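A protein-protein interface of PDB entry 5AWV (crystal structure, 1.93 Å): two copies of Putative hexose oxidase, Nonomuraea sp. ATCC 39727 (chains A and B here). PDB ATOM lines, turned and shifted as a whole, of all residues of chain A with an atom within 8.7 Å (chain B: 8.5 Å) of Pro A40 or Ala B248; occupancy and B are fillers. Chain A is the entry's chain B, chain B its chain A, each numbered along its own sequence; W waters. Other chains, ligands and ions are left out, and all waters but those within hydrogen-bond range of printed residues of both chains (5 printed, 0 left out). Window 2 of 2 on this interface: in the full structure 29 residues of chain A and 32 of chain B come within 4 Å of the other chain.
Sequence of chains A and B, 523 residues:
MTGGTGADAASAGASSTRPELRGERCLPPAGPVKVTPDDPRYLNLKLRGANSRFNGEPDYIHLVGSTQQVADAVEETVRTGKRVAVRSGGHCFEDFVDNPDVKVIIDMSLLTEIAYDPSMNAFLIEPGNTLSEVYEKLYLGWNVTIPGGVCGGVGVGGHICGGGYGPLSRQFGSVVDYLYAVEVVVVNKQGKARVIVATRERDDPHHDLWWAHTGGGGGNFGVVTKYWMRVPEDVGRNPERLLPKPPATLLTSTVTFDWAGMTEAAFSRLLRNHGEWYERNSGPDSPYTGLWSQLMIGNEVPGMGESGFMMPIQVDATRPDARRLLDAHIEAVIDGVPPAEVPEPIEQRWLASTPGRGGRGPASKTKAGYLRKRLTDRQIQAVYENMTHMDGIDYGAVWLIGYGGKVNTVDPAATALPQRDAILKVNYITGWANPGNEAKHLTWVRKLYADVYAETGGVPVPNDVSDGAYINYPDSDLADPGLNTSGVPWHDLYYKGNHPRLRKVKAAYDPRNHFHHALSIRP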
ATOM      1  N   VAL A  35      -4.404   5.134 -14.681  1.00  0.00           N
ATOM      2  CA  VAL A  35      -5.641   5.417 -15.418  1.00  0.00           C
ATOM      3  C   VAL A  35      -6.811   5.250 -14.438  1.00  0.00           C
ATOM      4  O   VAL A  35      -7.189   4.146 -14.069  1.00  0.00           O
ATOM      5  CB  VAL A  35      -5.738   4.524 -16.682  1.00  0.00           C
ATOM      6  CG1 VAL A  35      -6.998   4.819 -17.466  1.00  0.00           C
ATOM      7  CG2 VAL A  35      -4.484   4.723 -17.572  1.00  0.00           C
ATOM      8  N   THR A  36      -7.425   6.366 -14.082  1.00  0.00           N
ATOM      9  CA  THR A  36      -8.606   6.371 -13.229  1.00  0.00           C
ATOM     10  C   THR A  36      -9.861   6.466 -14.066  1.00  0.00           C
ATOM     11  O   THR A  36      -9.814   6.767 -15.263  1.00  0.00           O
ATOM     12  CB  THR A  36      -8.548   7.555 -12.247  1.00  0.00           C
ATOM     13  OG1 THR A  36      -8.527   8.763 -13.010  1.00  0.00           O
ATOM     14  CG2 THR A  36      -7.327   7.517 -11.394  1.00  0.00           C
ATOM     15  N   PRO A  37     -11.018   6.240 -13.443  1.00  0.00           N
ATOM     16  CA  PRO A  37     -12.259   6.214 -14.212  1.00  0.00           C
ATOM     17  C   PRO A  37     -12.636   7.440 -15.007  1.00  0.00           C
ATOM     18  O   PRO A  37     -13.415   7.295 -15.956  1.00  0.00           O
ATOM     19  CB  PRO A  37     -13.299   5.934 -13.162  1.00  0.00           C
ATOM     20  CG  PRO A  37     -12.590   5.161 -12.163  1.00  0.00           C
ATOM     21  CD  PRO A  37     -11.269   5.807 -12.054  1.00  0.00           C
ATOM     22  N   ASP A  38     -12.098   8.589 -14.691  1.00  0.00           N
ATOM     23  CA  ASP A  38     -12.366   9.737 -15.543  1.00  0.00           C
ATOM     24  C   ASP A  38     -11.386   9.914 -16.700  1.00  0.00           C
ATOM     25  O   ASP A  38     -11.442  10.916 -17.385  1.00  0.00           O
ATOM     26  CB  ASP A  38     -12.431  11.013 -14.739  1.00  0.00           C
ATOM     27  CG  ASP A  38     -11.172  11.298 -13.991  1.00  0.00           C
ATOM     28  OD1 ASP A  38     -10.498  10.355 -13.516  1.00  0.00           O
ATOM     29  OD2 ASP A  38     -10.875  12.468 -13.829  1.00  0.00           O
ATOM     30  N   ASP A  39     -10.485   8.966 -16.911  1.00  0.00           N
ATOM     31  CA  ASP A  39      -9.470   9.108 -17.937  1.00  0.00           C
ATOM     32  C   ASP A  39     -10.095   8.440 -19.138  1.00  0.00           C
ATOM     33  O   ASP A  39     -10.782   7.443 -19.035  1.00  0.00           O
ATOM     34  CB  ASP A  39      -8.141   8.476 -17.449  1.00  0.00           C
ATOM     35  CG  ASP A  39      -7.033   8.538 -18.461  1.00  0.00           C
ATOM     36  OD1 ASP A  39      -7.124   7.878 -19.528  1.00  0.00           O
ATOM     37  OD2 ASP A  39      -6.051   9.214 -18.183  1.00  0.00           O
ATOM     38  N   PRO A  40      -9.873   9.014 -20.322  1.00  0.00           N
ATOM     39  CA  PRO A  40     -10.514   8.439 -21.469  1.00  0.00           C
ATOM     40  C   PRO A  40     -10.082   7.011 -21.820  1.00  0.00           C
ATOM     41  O   PRO A  40     -10.831   6.369 -22.486  1.00  0.00           O
ATOM     42  CB  PRO A  40     -10.138   9.413 -22.598  1.00  0.00           C
ATOM     43  CG  PRO A  40      -8.933  10.071 -22.184  1.00  0.00           C
ATOM     44  CD  PRO A  40      -9.125  10.252 -20.678  1.00  0.00           C
ATOM     45  N   ARG A  41      -8.877   6.603 -21.415  1.00  0.00           N
ATOM     46  CA  ARG A  41      -8.374   5.221 -21.607  1.00  0.00           C
ATOM     47  C   ARG A  41      -8.999   4.197 -20.682  1.00  0.00           C
ATOM     48  O   ARG A  41      -8.789   3.005 -20.892  1.00  0.00           O
ATOM     49  CB  ARG A  41      -6.867   5.223 -21.385  1.00  0.00           C
ATOM     50  CG  ARG A  41      -6.107   6.032 -22.381  1.00  0.00           C
ATOM     51  CD  ARG A  41      -4.673   6.275 -21.974  1.00  0.00           C
ATOM     52  NE  ARG A  41      -4.587   7.299 -20.968  1.00  0.00           N
ATOM     53  CZ  ARG A  41      -3.495   7.955 -20.664  1.00  0.00           C
ATOM     54  NH1 ARG A  41      -2.314   7.681 -21.248  1.00  0.00           N
ATOM     55  NH2 ARG A  41      -3.571   8.856 -19.722  1.00  0.00           N
ATOM     56  N   TYR A  42      -9.756   4.638 -19.643  1.00  0.00           N
ATOM     57  CA  TYR A  42     -10.213   3.737 -18.624  1.00  0.00           C
ATOM     58  C   TYR A  42     -11.075   2.577 -19.166  1.00  0.00           C
ATOM     59  O   TYR A  42     -10.746   1.413 -18.939  1.00  0.00           O
ATOM     60  CB  TYR A  42     -10.902   4.480 -17.467  1.00  0.00           C
ATOM     61  CG  TYR A  42     -11.375   3.541 -16.354  1.00  0.00           C
ATOM     62  CD1 TYR A  42     -10.526   3.138 -15.342  1.00  0.00           C
ATOM     63  CD2 TYR A  42     -12.699   3.186 -16.258  1.00  0.00           C
ATOM     64  CE1 TYR A  42     -11.021   2.366 -14.282  1.00  0.00           C
ATOM     65  CE2 TYR A  42     -13.169   2.387 -15.236  1.00  0.00           C
ATOM     66  CZ  TYR A  42     -12.341   1.997 -14.250  1.00  0.00           C
ATOM     67  OH  TYR A  42     -12.827   1.122 -13.273  1.00  0.00           O
ATOM     68  N   LEU A  43     -12.114   2.863 -19.917  1.00  0.00           N
ATOM     69  CA  LEU A  43     -13.027   1.798 -20.372  1.00  0.00           C
ATOM     70  C   LEU A  43     -12.341   0.789 -21.312  1.00  0.00           C
ATOM     71  O   LEU A  43     -12.469  -0.424 -21.204  1.00  0.00           O
ATOM     72  CB  LEU A  43     -14.313   2.436 -21.001  1.00  0.00           C
ATOM     73  CG  LEU A  43     -15.270   2.944 -19.912  1.00  0.00           C
ATOM     74  CD1 LEU A  43     -16.412   3.870 -20.394  1.00  0.00           C
ATOM     75  CD2 LEU A  43     -15.815   1.780 -19.063  1.00  0.00           C
ATOM     76  N   ASN A  44     -11.540   1.299 -22.238  1.00  0.00           N
ATOM     77  CA  ASN A  44     -10.757   0.451 -23.115  1.00  0.00           C
ATOM     78  C   ASN A  44      -9.933  -0.601 -22.306  1.00  0.00           C
ATOM     79  O   ASN A  44     -10.024  -1.802 -22.585  1.00  0.00           O
ATOM     80  CB  ASN A  44      -9.824   1.307 -23.968  1.00  0.00           C
ATOM     81  CG  ASN A  44     -10.512   1.893 -25.164  1.00  0.00           C
ATOM     82  OD1 ASN A  44     -11.759   1.801 -25.344  1.00  0.00           O
ATOM     83  ND2 ASN A  44      -9.716   2.473 -26.022  1.00  0.00           N
ATOM     84  N   LEU A  45      -9.257  -0.136 -21.271  1.00  0.00           N
ATOM     85  CA  LEU A  45      -8.390  -0.989 -20.466  1.00  0.00           C
ATOM     86  C   LEU A  45      -9.223  -1.880 -19.552  1.00  0.00           C
ATOM     87  O   LEU A  45      -8.929  -3.042 -19.359  1.00  0.00           O
ATOM     88  CB  LEU A  45      -7.396  -0.162 -19.654  1.00  0.00           C
ATOM     89  CG  LEU A  45      -6.335   0.472 -20.568  1.00  0.00           C
ATOM     90  CD1 LEU A  45      -5.485   1.449 -19.803  1.00  0.00           C
ATOM     91  CD2 LEU A  45      -5.478  -0.516 -21.328  1.00  0.00           C
ATOM     92  N   LYS A  46     -10.299  -1.330 -18.990  1.00  0.00           N
ATOM     93  CA  LYS A  46     -11.255  -2.170 -18.156  1.00  0.00           C
ATOM     94  C   LYS A  46     -11.902  -3.290 -18.966  1.00  0.00           C
ATOM     95  O   LYS A  46     -12.202  -4.358 -18.457  1.00  0.00           O
ATOM     96  CB  LYS A  46     -12.315  -1.262 -17.556  1.00  0.00           C
ATOM     97  CG  LYS A  46     -13.142  -1.833 -16.402  1.00  0.00           C
ATOM     98  CD  LYS A  46     -14.295  -0.909 -16.131  1.00  0.00           C
ATOM     99  CE  LYS A  46     -15.486  -1.300 -16.980  1.00  0.00           C
ATOM    100  NZ  LYS A  46     -16.257  -2.463 -16.436  1.00  0.00           N
ATOM    101  N   TYR B 139      -1.635   6.516 -27.878  1.00  0.00           N
ATOM    102  CA  TYR B 139      -2.789   6.693 -27.023  1.00  0.00           C
ATOM    103  C   TYR B 139      -2.611   6.152 -25.601  1.00  0.00           C
ATOM    104  O   TYR B 139      -2.783   6.929 -24.616  1.00  0.00           O
ATOM    105  CB  TYR B 139      -3.984   6.002 -27.630  1.00  0.00           C
ATOM    106  CG  TYR B 139      -5.327   6.258 -26.921  1.00  0.00           C
ATOM    107  CD1 TYR B 139      -5.671   7.522 -26.499  1.00  0.00           C
ATOM    108  CD2 TYR B 139      -6.183   5.207 -26.563  1.00  0.00           C
ATOM    109  CE1 TYR B 139      -6.882   7.774 -25.896  1.00  0.00           C
ATOM    110  CE2 TYR B 139      -7.395   5.455 -25.898  1.00  0.00           C
ATOM    111  CZ  TYR B 139      -7.755   6.756 -25.623  1.00  0.00           C
ATOM    112  OH  TYR B 139      -8.968   7.109 -25.009  1.00  0.00           O
ATOM    113  N   LEU B 140      -2.151   4.904 -25.509  1.00  0.00           N
ATOM    114  CA  LEU B 140      -1.869   4.282 -24.182  1.00  0.00           C
ATOM    115  C   LEU B 140      -0.799   5.015 -23.342  1.00  0.00           C
ATOM    116  O   LEU B 140      -1.017   5.320 -22.131  1.00  0.00           O
ATOM    117  CB  LEU B 140      -1.628   2.782 -24.310  1.00  0.00           C
ATOM    118  CG  LEU B 140      -2.883   1.990 -24.717  1.00  0.00           C
ATOM    119  CD1 LEU B 140      -2.647   0.498 -24.577  1.00  0.00           C
ATOM    120  CD2 LEU B 140      -4.159   2.318 -23.925  1.00  0.00           C
ATOM    121  N   TRP B 142       0.606   8.155 -23.802  1.00  0.00           N
ATOM    122  CA  TRP B 142       0.601   9.624 -23.595  1.00  0.00           C
ATOM    123  C   TRP B 142      -0.749  10.323 -23.914  1.00  0.00           C
ATOM    124  O   TRP B 142      -0.844  11.524 -23.792  1.00  0.00           O
ATOM    125  CB  TRP B 142       1.705  10.266 -24.451  1.00  0.00           C
ATOM    126  CG  TRP B 142       3.066   9.720 -24.172  1.00  0.00           C
ATOM    127  CD1 TRP B 142       3.931  10.147 -23.206  1.00  0.00           C
ATOM    128  CD2 TRP B 142       3.702   8.611 -24.807  1.00  0.00           C
ATOM    129  NE1 TRP B 142       5.036   9.373 -23.212  1.00  0.00           N
ATOM    130  CE2 TRP B 142       4.941   8.446 -24.203  1.00  0.00           C
ATOM    131  CE3 TRP B 142       3.356   7.766 -25.866  1.00  0.00           C
ATOM    132  CZ2 TRP B 142       5.811   7.470 -24.587  1.00  0.00           C
ATOM    133  CZ3 TRP B 142       4.192   6.832 -26.253  1.00  0.00           C
ATOM    134  CH2 TRP B 142       5.424   6.656 -25.611  1.00  0.00           C
ATOM    135  N   ASN B 143      -1.786   9.562 -24.263  1.00  0.00           N
ATOM    136  CA  ASN B 143      -3.053  10.122 -24.716  1.00  0.00           C
ATOM    137  C   ASN B 143      -2.876  11.148 -25.842  1.00  0.00           C
ATOM    138  O   ASN B 143      -3.396  12.280 -25.755  1.00  0.00           O
ATOM    139  CB  ASN B 143      -3.732  10.758 -23.510  1.00  0.00           C
ATOM    140  CG  ASN B 143      -5.102  11.178 -23.770  1.00  0.00           C
ATOM    141  OD1 ASN B 143      -5.800  10.699 -24.686  1.00  0.00           O
ATOM    142  ND2 ASN B 143      -5.544  12.131 -22.953  1.00  0.00           N
ATOM    143  N   VAL B 144      -2.084  10.762 -26.838  1.00  0.00           N
ATOM    144  CA  VAL B 144      -1.855  11.580 -28.042  1.00  0.00           C
ATOM    145  C   VAL B 144      -2.165  10.732 -29.266  1.00  0.00           C
ATOM    146  O   VAL B 144      -2.458   9.544 -29.152  1.00  0.00           O
ATOM    147  CB  VAL B 144      -0.499  12.247 -28.108  1.00  0.00           C
ATOM    148  CG1 VAL B 144      -0.288  13.194 -26.908  1.00  0.00           C
ATOM    149  CG2 VAL B 144       0.681  11.243 -28.217  1.00  0.00           C
ATOM    150  N   GLU B 240       2.831  14.511 -23.113  1.00  0.00           N
ATOM    151  CA  GLU B 240       1.372  14.564 -23.343  1.00  0.00           C
ATOM    152  C   GLU B 240       0.874  15.758 -24.116  1.00  0.00           C
ATOM    153  O   GLU B 240      -0.267  15.764 -24.536  1.00  0.00           O
ATOM    154  CB  GLU B 240       0.604  14.458 -22.029  1.00  0.00           C
ATOM    155  CG  GLU B 240       0.840  13.208 -21.228  1.00  0.00           C
ATOM    156  CD  GLU B 240      -0.221  13.113 -20.123  1.00  0.00           C
ATOM    157  OE1 GLU B 240       0.043  13.606 -19.005  1.00  0.00           O
ATOM    158  OE2 GLU B 240      -1.342  12.627 -20.416  1.00  0.00           O
ATOM    159  N   LYS B 245      -4.249  15.679 -28.961  1.00  0.00           N
ATOM    160  CA  LYS B 245      -4.953  14.831 -28.069  1.00  0.00           C
ATOM    161  C   LYS B 245      -6.175  14.298 -28.805  1.00  0.00           C
ATOM    162  O   LYS B 245      -6.935  15.104 -29.296  1.00  0.00           O
ATOM    163  CB  LYS B 245      -5.394  15.641 -26.855  1.00  0.00           C
ATOM    164  CG  LYS B 245      -6.150  14.796 -25.794  1.00  0.00           C
ATOM    165  CD  LYS B 245      -6.535  15.592 -24.523  1.00  0.00           C
ATOM    166  CE  LYS B 245      -5.422  16.549 -24.018  1.00  0.00           C
ATOM    167  NZ  LYS B 245      -4.729  16.247 -22.707  1.00  0.00           N
ATOM    168  N   PRO B 246      -6.333  12.955 -28.940  1.00  0.00           N
ATOM    169  CA  PRO B 246      -7.565  12.527 -29.653  1.00  0.00           C
ATOM    170  C   PRO B 246      -8.848  12.847 -28.844  1.00  0.00           C
ATOM    171  O   PRO B 246      -8.806  13.087 -27.629  1.00  0.00           O
ATOM    172  CB  PRO B 246      -7.380  10.992 -29.793  1.00  0.00           C
ATOM    173  CG  PRO B 246      -6.658  10.640 -28.539  1.00  0.00           C
ATOM    174  CD  PRO B 246      -5.675  11.802 -28.305  1.00  0.00           C
ATOM    175  N   PRO B 247      -9.975  12.914 -29.526  1.00  0.00           N
ATOM    176  CA  PRO B 247     -11.214  13.046 -28.806  1.00  0.00           C
ATOM    177  C   PRO B 247     -11.441  11.780 -27.932  1.00  0.00           C
ATOM    178  O   PRO B 247     -11.169  10.660 -28.411  1.00  0.00           O
ATOM    179  CB  PRO B 247     -12.289  13.080 -29.911  1.00  0.00           C
ATOM    180  CG  PRO B 247     -11.590  12.825 -31.142  1.00  0.00           C
ATOM    181  CD  PRO B 247     -10.130  12.929 -30.978  1.00  0.00           C
ATOM    182  N   ALA B 248     -11.966  11.966 -26.733  1.00  0.00           N
ATOM    183  CA  ALA B 248     -12.370  10.836 -25.903  1.00  0.00           C
ATOM    184  C   ALA B 248     -13.407   9.959 -26.587  1.00  0.00           C
ATOM    185  O   ALA B 248     -13.305   8.718 -26.566  1.00  0.00           O
ATOM    186  CB  ALA B 248     -12.924  11.345 -24.604  1.00  0.00           C
ATOM    187  N   THR B 249     -14.365  10.614 -27.281  1.00  0.00           N
ATOM    188  CA  THR B 249     -15.450   9.939 -27.958  1.00  0.00           C
ATOM    189  C   THR B 249     -15.848  10.650 -29.237  1.00  0.00           C
ATOM    190  O   THR B 249     -15.601  11.846 -29.381  1.00  0.00           O
ATOM    191  CB  THR B 249     -16.718   9.835 -27.086  1.00  0.00           C
ATOM    192  OG1 THR B 249     -17.156  11.117 -26.815  1.00  0.00           O
ATOM    193  CG2 THR B 249     -16.457   9.174 -25.746  1.00  0.00           C
ATOM    194  N   LEU B 250     -16.387   9.843 -30.161  1.00  0.00           N
ATOM    195  CA  LEU B 250     -16.898  10.284 -31.436  1.00  0.00           C
ATOM    196  C   LEU B 250     -18.386   9.971 -31.509  1.00  0.00           C
ATOM    197  O   LEU B 250     -18.827   8.892 -31.029  1.00  0.00           O
ATOM    198  CB  LEU B 250     -16.181   9.543 -32.560  1.00  0.00           C
ATOM    199  CG  LEU B 250     -14.669   9.822 -32.623  1.00  0.00           C
ATOM    200  CD1 LEU B 250     -14.003   8.740 -33.479  1.00  0.00           C
ATOM    201  CD2 LEU B 250     -14.343  11.190 -33.212  1.00  0.00           C
ATOM    202  N   LEU B 251     -19.138  10.892 -32.068  1.00  0.00           N
ATOM    203  CA  LEU B 251     -20.460  10.550 -32.564  1.00  0.00           C
ATOM    204  C   LEU B 251     -20.386  10.120 -34.017  1.00  0.00           C
ATOM    205  O   LEU B 251     -19.820  10.808 -34.880  1.00  0.00           O
ATOM    206  CB  LEU B 251     -21.363  11.782 -32.334  1.00  0.00           C
ATOM    207  CG  LEU B 251     -22.858  11.716 -32.135  1.00  0.00           C
ATOM    208  CD1 LEU B 251     -23.241  10.733 -31.018  1.00  0.00           C
ATOM    209  CD2 LEU B 251     -23.363  13.134 -31.804  1.00  0.00           C
ATOM    210  N   VAL B 315     -18.079  12.783 -35.778  1.00  0.00           N
ATOM    211  CA  VAL B 315     -17.826  14.085 -35.201  1.00  0.00           C
ATOM    212  C   VAL B 315     -17.245  13.909 -33.828  1.00  0.00           C
ATOM    213  O   VAL B 315     -17.652  13.006 -33.096  1.00  0.00           O
ATOM    214  CB  VAL B 315     -19.155  14.867 -35.066  1.00  0.00           C
ATOM    215  CG1 VAL B 315     -18.961  16.300 -34.607  1.00  0.00           C
ATOM    216  CG2 VAL B 315     -19.806  14.887 -36.422  1.00  0.00           C
ATOM    217  N   ASP B 316     -16.270  14.750 -33.507  1.00  0.00           N
ATOM    218  CA  ASP B 316     -15.740  14.893 -32.159  1.00  0.00           C
ATOM    219  C   ASP B 316     -16.890  15.202 -31.215  1.00  0.00           C
ATOM    220  O   ASP B 316     -17.506  16.260 -31.322  1.00  0.00           O
ATOM    221  CB  ASP B 316     -14.729  16.049 -32.160  1.00  0.00           C
ATOM    222  CG  ASP B 316     -14.090  16.292 -30.805  1.00  0.00           C
ATOM    223  OD1 ASP B 316     -14.502  15.692 -29.778  1.00  0.00           O
ATOM    224  OD2 ASP B 316     -13.087  17.004 -30.824  1.00  0.00           O
ATOM    225  N   ALA B 317     -17.163  14.279 -30.315  1.00  0.00           N
ATOM    226  CA  ALA B 317     -18.216  14.363 -29.339  1.00  0.00           C
ATOM    227  C   ALA B 317     -17.904  15.135 -28.047  1.00  0.00           C
ATOM    228  O   ALA B 317     -18.722  15.140 -27.163  1.00  0.00           O
ATOM    229  CB  ALA B 317     -18.694  12.967 -29.006  1.00  0.00           C
ATOM    230  N   THR B 318     -16.770  15.814 -27.954  1.00  0.00           N
ATOM    231  CA  THR B 318     -16.367  16.557 -26.784  1.00  0.00           C
ATOM    232  C   THR B 318     -17.325  17.750 -26.491  1.00  0.00           C
ATOM    233  O   THR B 318     -17.741  17.930 -25.348  1.00  0.00           O
ATOM    234  CB  THR B 318     -14.996  17.184 -27.021  1.00  0.00           C
ATOM    235  OG1 THR B 318     -14.075  16.166 -27.308  1.00  0.00           O
ATOM    236  CG2 THR B 318     -14.476  18.066 -25.806  1.00  0.00           C
ATOM    237  N   GLU B 347     -22.444   6.882 -30.040  1.00  0.00           N
ATOM    238  CA  GLU B 347     -21.243   7.469 -29.450  1.00  0.00           C
ATOM    239  C   GLU B 347     -20.212   6.367 -29.250  1.00  0.00           C
ATOM    240  O   GLU B 347     -20.548   5.311 -28.723  1.00  0.00           O
ATOM    241  CB  GLU B 347     -21.568   8.193 -28.164  1.00  0.00           C
ATOM    242  CG  GLU B 347     -20.377   8.904 -27.576  1.00  0.00           C
ATOM    243  CD  GLU B 347     -20.736   9.938 -26.532  1.00  0.00           C
ATOM    244  OE1 GLU B 347     -19.816  10.538 -25.933  1.00  0.00           O
ATOM    245  OE2 GLU B 347     -21.933  10.166 -26.313  1.00  0.00           O
ATOM    246  N   GLN B 348     -19.025   6.514 -29.825  1.00  0.00           N
ATOM    247  CA  GLN B 348     -17.949   5.483 -29.686  1.00  0.00           C
ATOM    248  C   GLN B 348     -16.704   6.058 -29.048  1.00  0.00           C
ATOM    249  O   GLN B 348     -16.324   7.162 -29.360  1.00  0.00           O
ATOM    250  CB  GLN B 348     -17.533   5.008 -31.064  1.00  0.00           C
ATOM    251  CG  GLN B 348     -18.713   4.577 -31.893  1.00  0.00           C
ATOM    252  CD  GLN B 348     -18.297   3.664 -33.000  1.00  0.00           C
ATOM    253  OE1 GLN B 348     -17.835   2.564 -32.744  1.00  0.00           O
ATOM    254  NE2 GLN B 348     -18.438   4.102 -34.217  1.00  0.00           N
ATOM    255  N   ARG B 349     -16.029   5.274 -28.212  1.00  0.00           N
ATOM    256  CA  ARG B 349     -14.818   5.706 -27.602  1.00  0.00           C
ATOM    257  C   ARG B 349     -13.667   5.616 -28.628  1.00  0.00           C
ATOM    258  O   ARG B 349     -13.674   4.765 -29.491  1.00  0.00           O
ATOM    259  CB  ARG B 349     -14.454   4.833 -26.405  1.00  0.00           C
ATOM    260  CG  ARG B 349     -15.502   4.728 -25.299  1.00  0.00           C
ATOM    261  CD  ARG B 349     -14.854   3.975 -24.114  1.00  0.00           C
ATOM    262  NE  ARG B 349     -14.341   2.633 -24.464  1.00  0.00           N
ATOM    263  CZ  ARG B 349     -15.068   1.521 -24.540  1.00  0.00           C
ATOM    264  NH1 ARG B 349     -16.385   1.534 -24.349  1.00  0.00           N
ATOM    265  NH2 ARG B 349     -14.500   0.394 -24.900  1.00  0.00           N
ATOM    266  N   TRP B 350     -12.674   6.450 -28.450  1.00  0.00           N
ATOM    267  CA  TRP B 350     -11.490   6.398 -29.265  1.00  0.00           C
ATOM    268  C   TRP B 350     -10.817   5.026 -29.148  1.00  0.00           C
ATOM    269  O   TRP B 350     -10.614   4.498 -28.030  1.00  0.00           O
ATOM    270  CB  TRP B 350     -10.542   7.481 -28.811  1.00  0.00           C
ATOM    271  CG  TRP B 350      -9.339   7.602 -29.658  1.00  0.00           C
ATOM    272  CD1 TRP B 350      -8.028   7.195 -29.378  1.00  0.00           C
ATOM    273  CD2 TRP B 350      -9.321   8.176 -30.924  1.00  0.00           C
ATOM    274  NE1 TRP B 350      -7.195   7.515 -30.437  1.00  0.00           N
ATOM    275  CE2 TRP B 350      -7.977   8.068 -31.421  1.00  0.00           C
ATOM    276  CE3 TRP B 350     -10.318   8.671 -31.751  1.00  0.00           C
ATOM    277  CZ2 TRP B 350      -7.614   8.520 -32.679  1.00  0.00           C
ATOM    278  CZ3 TRP B 350      -9.942   9.144 -33.009  1.00  0.00           C
ATOM    279  CH2 TRP B 350      -8.622   9.043 -33.464  1.00  0.00           C
ATOM    280  N   LEU B 351     -10.521   4.467 -30.312  1.00  0.00           N
ATOM    281  CA  LEU B 351      -9.926   3.189 -30.501  1.00  0.00           C
ATOM    282  C   LEU B 351     -10.630   2.071 -29.746  1.00  0.00           C
ATOM    283  O   LEU B 351      -9.989   1.105 -29.315  1.00  0.00           O
ATOM    284  CB  LEU B 351      -8.430   3.205 -30.134  1.00  0.00           C
ATOM    285  CG  LEU B 351      -7.500   4.077 -30.984  1.00  0.00           C
ATOM    286  CD1 LEU B 351      -6.155   4.171 -30.314  1.00  0.00           C
ATOM    287  CD2 LEU B 351      -7.407   3.574 -32.409  1.00  0.00           C
ATOM    288  N   ALA B 352     -11.932   2.169 -29.620  1.00  0.00           N
ATOM    289  CA  ALA B 352     -12.671   1.059 -29.006  1.00  0.00           C
ATOM    290  C   ALA B 352     -12.539  -0.267 -29.724  1.00  0.00           C
ATOM    291  O   ALA B 352     -12.584  -1.263 -29.062  1.00  0.00           O
ATOM    292  CB  ALA B 352     -14.142   1.386 -28.792  1.00  0.00           C
HETATM  293  O   HOH W   1     -11.555   4.013 -23.192  1.00  0.00           O
HETATM  294  O   HOH W   2     -12.705  -1.408 -25.960  1.00  0.00           O
HETATM  295  O   HOH W   3     -10.996   5.396 -25.566  1.00  0.00           O
HETATM  296  O   HOH W   4     -12.917   7.407 -24.250  1.00  0.00           O
HETATM  297  O   HOH W   5      -0.543   9.783 -20.284  1.00  0.00           O
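The backbone carbonyl oxygen of Pro A40 is in hydrogen-bond range of the side-chain hydroxyl of Tyr B139, 3.2 Å away.
The backbone carbonyl oxygen of Trp B350 sits at hydrogen-bond distance from the side-chain amide nitrogen of Asn A44, at 3.0 Å.
O of Tyr B139 lies close to NH1 of Arg A41, at 3.5 Å.
The guanidinium group of Arg B349 lies within hydrogen-bond range of the side-chain amide oxygen of Asn A44 (2.9 Å).
The guanidinium group (NH1) of Arg A41 lies within hydrogen-bond range of the backbone carbonyl oxygen (O) of Leu B140 (2.8 Å).
The backbone NH of Tyr B139 sits at hydrogen-bond distance from the backbone carbonyl oxygen of Val B144, at 3.4 Å.
OD2 of Asp A39 is in salt-bridge range of NH2 of Arg A41 (2.9 Å).
The backbone carbonyl oxygen (O) of Ala B248 lies within hydrogen-bond range of the backbone NH (N) of Trp B350 (3.0 Å).
Ala B248 touches Pro A40.
Arg A41 touches Trp B142.
Arg A41 touches Asn B143.
Leu A43 touches Arg B349 (CB to NE, 3.5 Å).
Tyr B139 touches Asn A44 (CE2 to ND2, 3.8 Å).
ND2 of Asn A44 touches O of Leu B351 (3.6 Å).
Ala B352 touches Asn A44.
No residue of chain B comes within 4 Å of Asp A39.
Tyr A42 touches none of the printed residues of chain B.
Printed residues of chain B within 4 Å of Leu A43: Arg B349.
Of the printed residues of chain A, Tyr B139 touches Pro A40 (3.2 Å), Arg A41 (3.3 Å) and Asn A44 (3.8 Å).
Of the printed residues of chain A, Leu B140 touches Arg A41.
Ala B248 touches just one residue of chain A: Pro A40.
No residue of chain A comes within 4 Å of Thr B249.
Asp B316 touches none of the printed residues of chain A.
The nearest residue of chain B that does not touch Pro A40 is Asn B143 (4.04 Å).
Hydrophobic or aromatic side chains of chain A that line the printed part of chain B: Pro A40 and Leu A43.
Hydrophobic or aromatic side chains of chain B that line the printed part of chain A: Tyr B139 and Ala B248.
Among the printed residues, no Asp or Glu carboxylate lies within 4 Å of a Lys or Arg side-chain nitrogen of the other chain.
No position is printed for both chains.
Of the 12 pairs that touch across the chains among the printed residues, none has its exchanged pair printed and touching as well.
Water W1 lies within hydrogen-bond range of the backbone carbonyl oxygen (O) of Pro A40 (2.6 Å), the backbone NH (N) of Asn A44 (2.9 Å) and the guanidinium group (NE) of Arg B349 (3.4 Å).
Water W3 lies within hydrogen-bond range of O of Trp B350 (2.7 Å), OH of Tyr B139 (2.7 Å), ND2 of Asn A44 (3.2 Å) and O of Pro A40 (3.2 Å).
Water W4 bridges the backbone carbonyl oxygen (O) of Ala B248 and the backbone carbonyl oxygen (O) of Pro A40.
Water W2 lies within hydrogen-bond range of the guanidinium group (NH2) of Arg B349, the backbone carbonyl oxygen (O) of Ala B352 and the side-chain amide oxygen (OD1) of Asn A44.
Water W5 bridges the guanidinium group of Arg A41 (2.9 Å) and the side-chain carboxylate of Glu B240 (3.0 Å).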
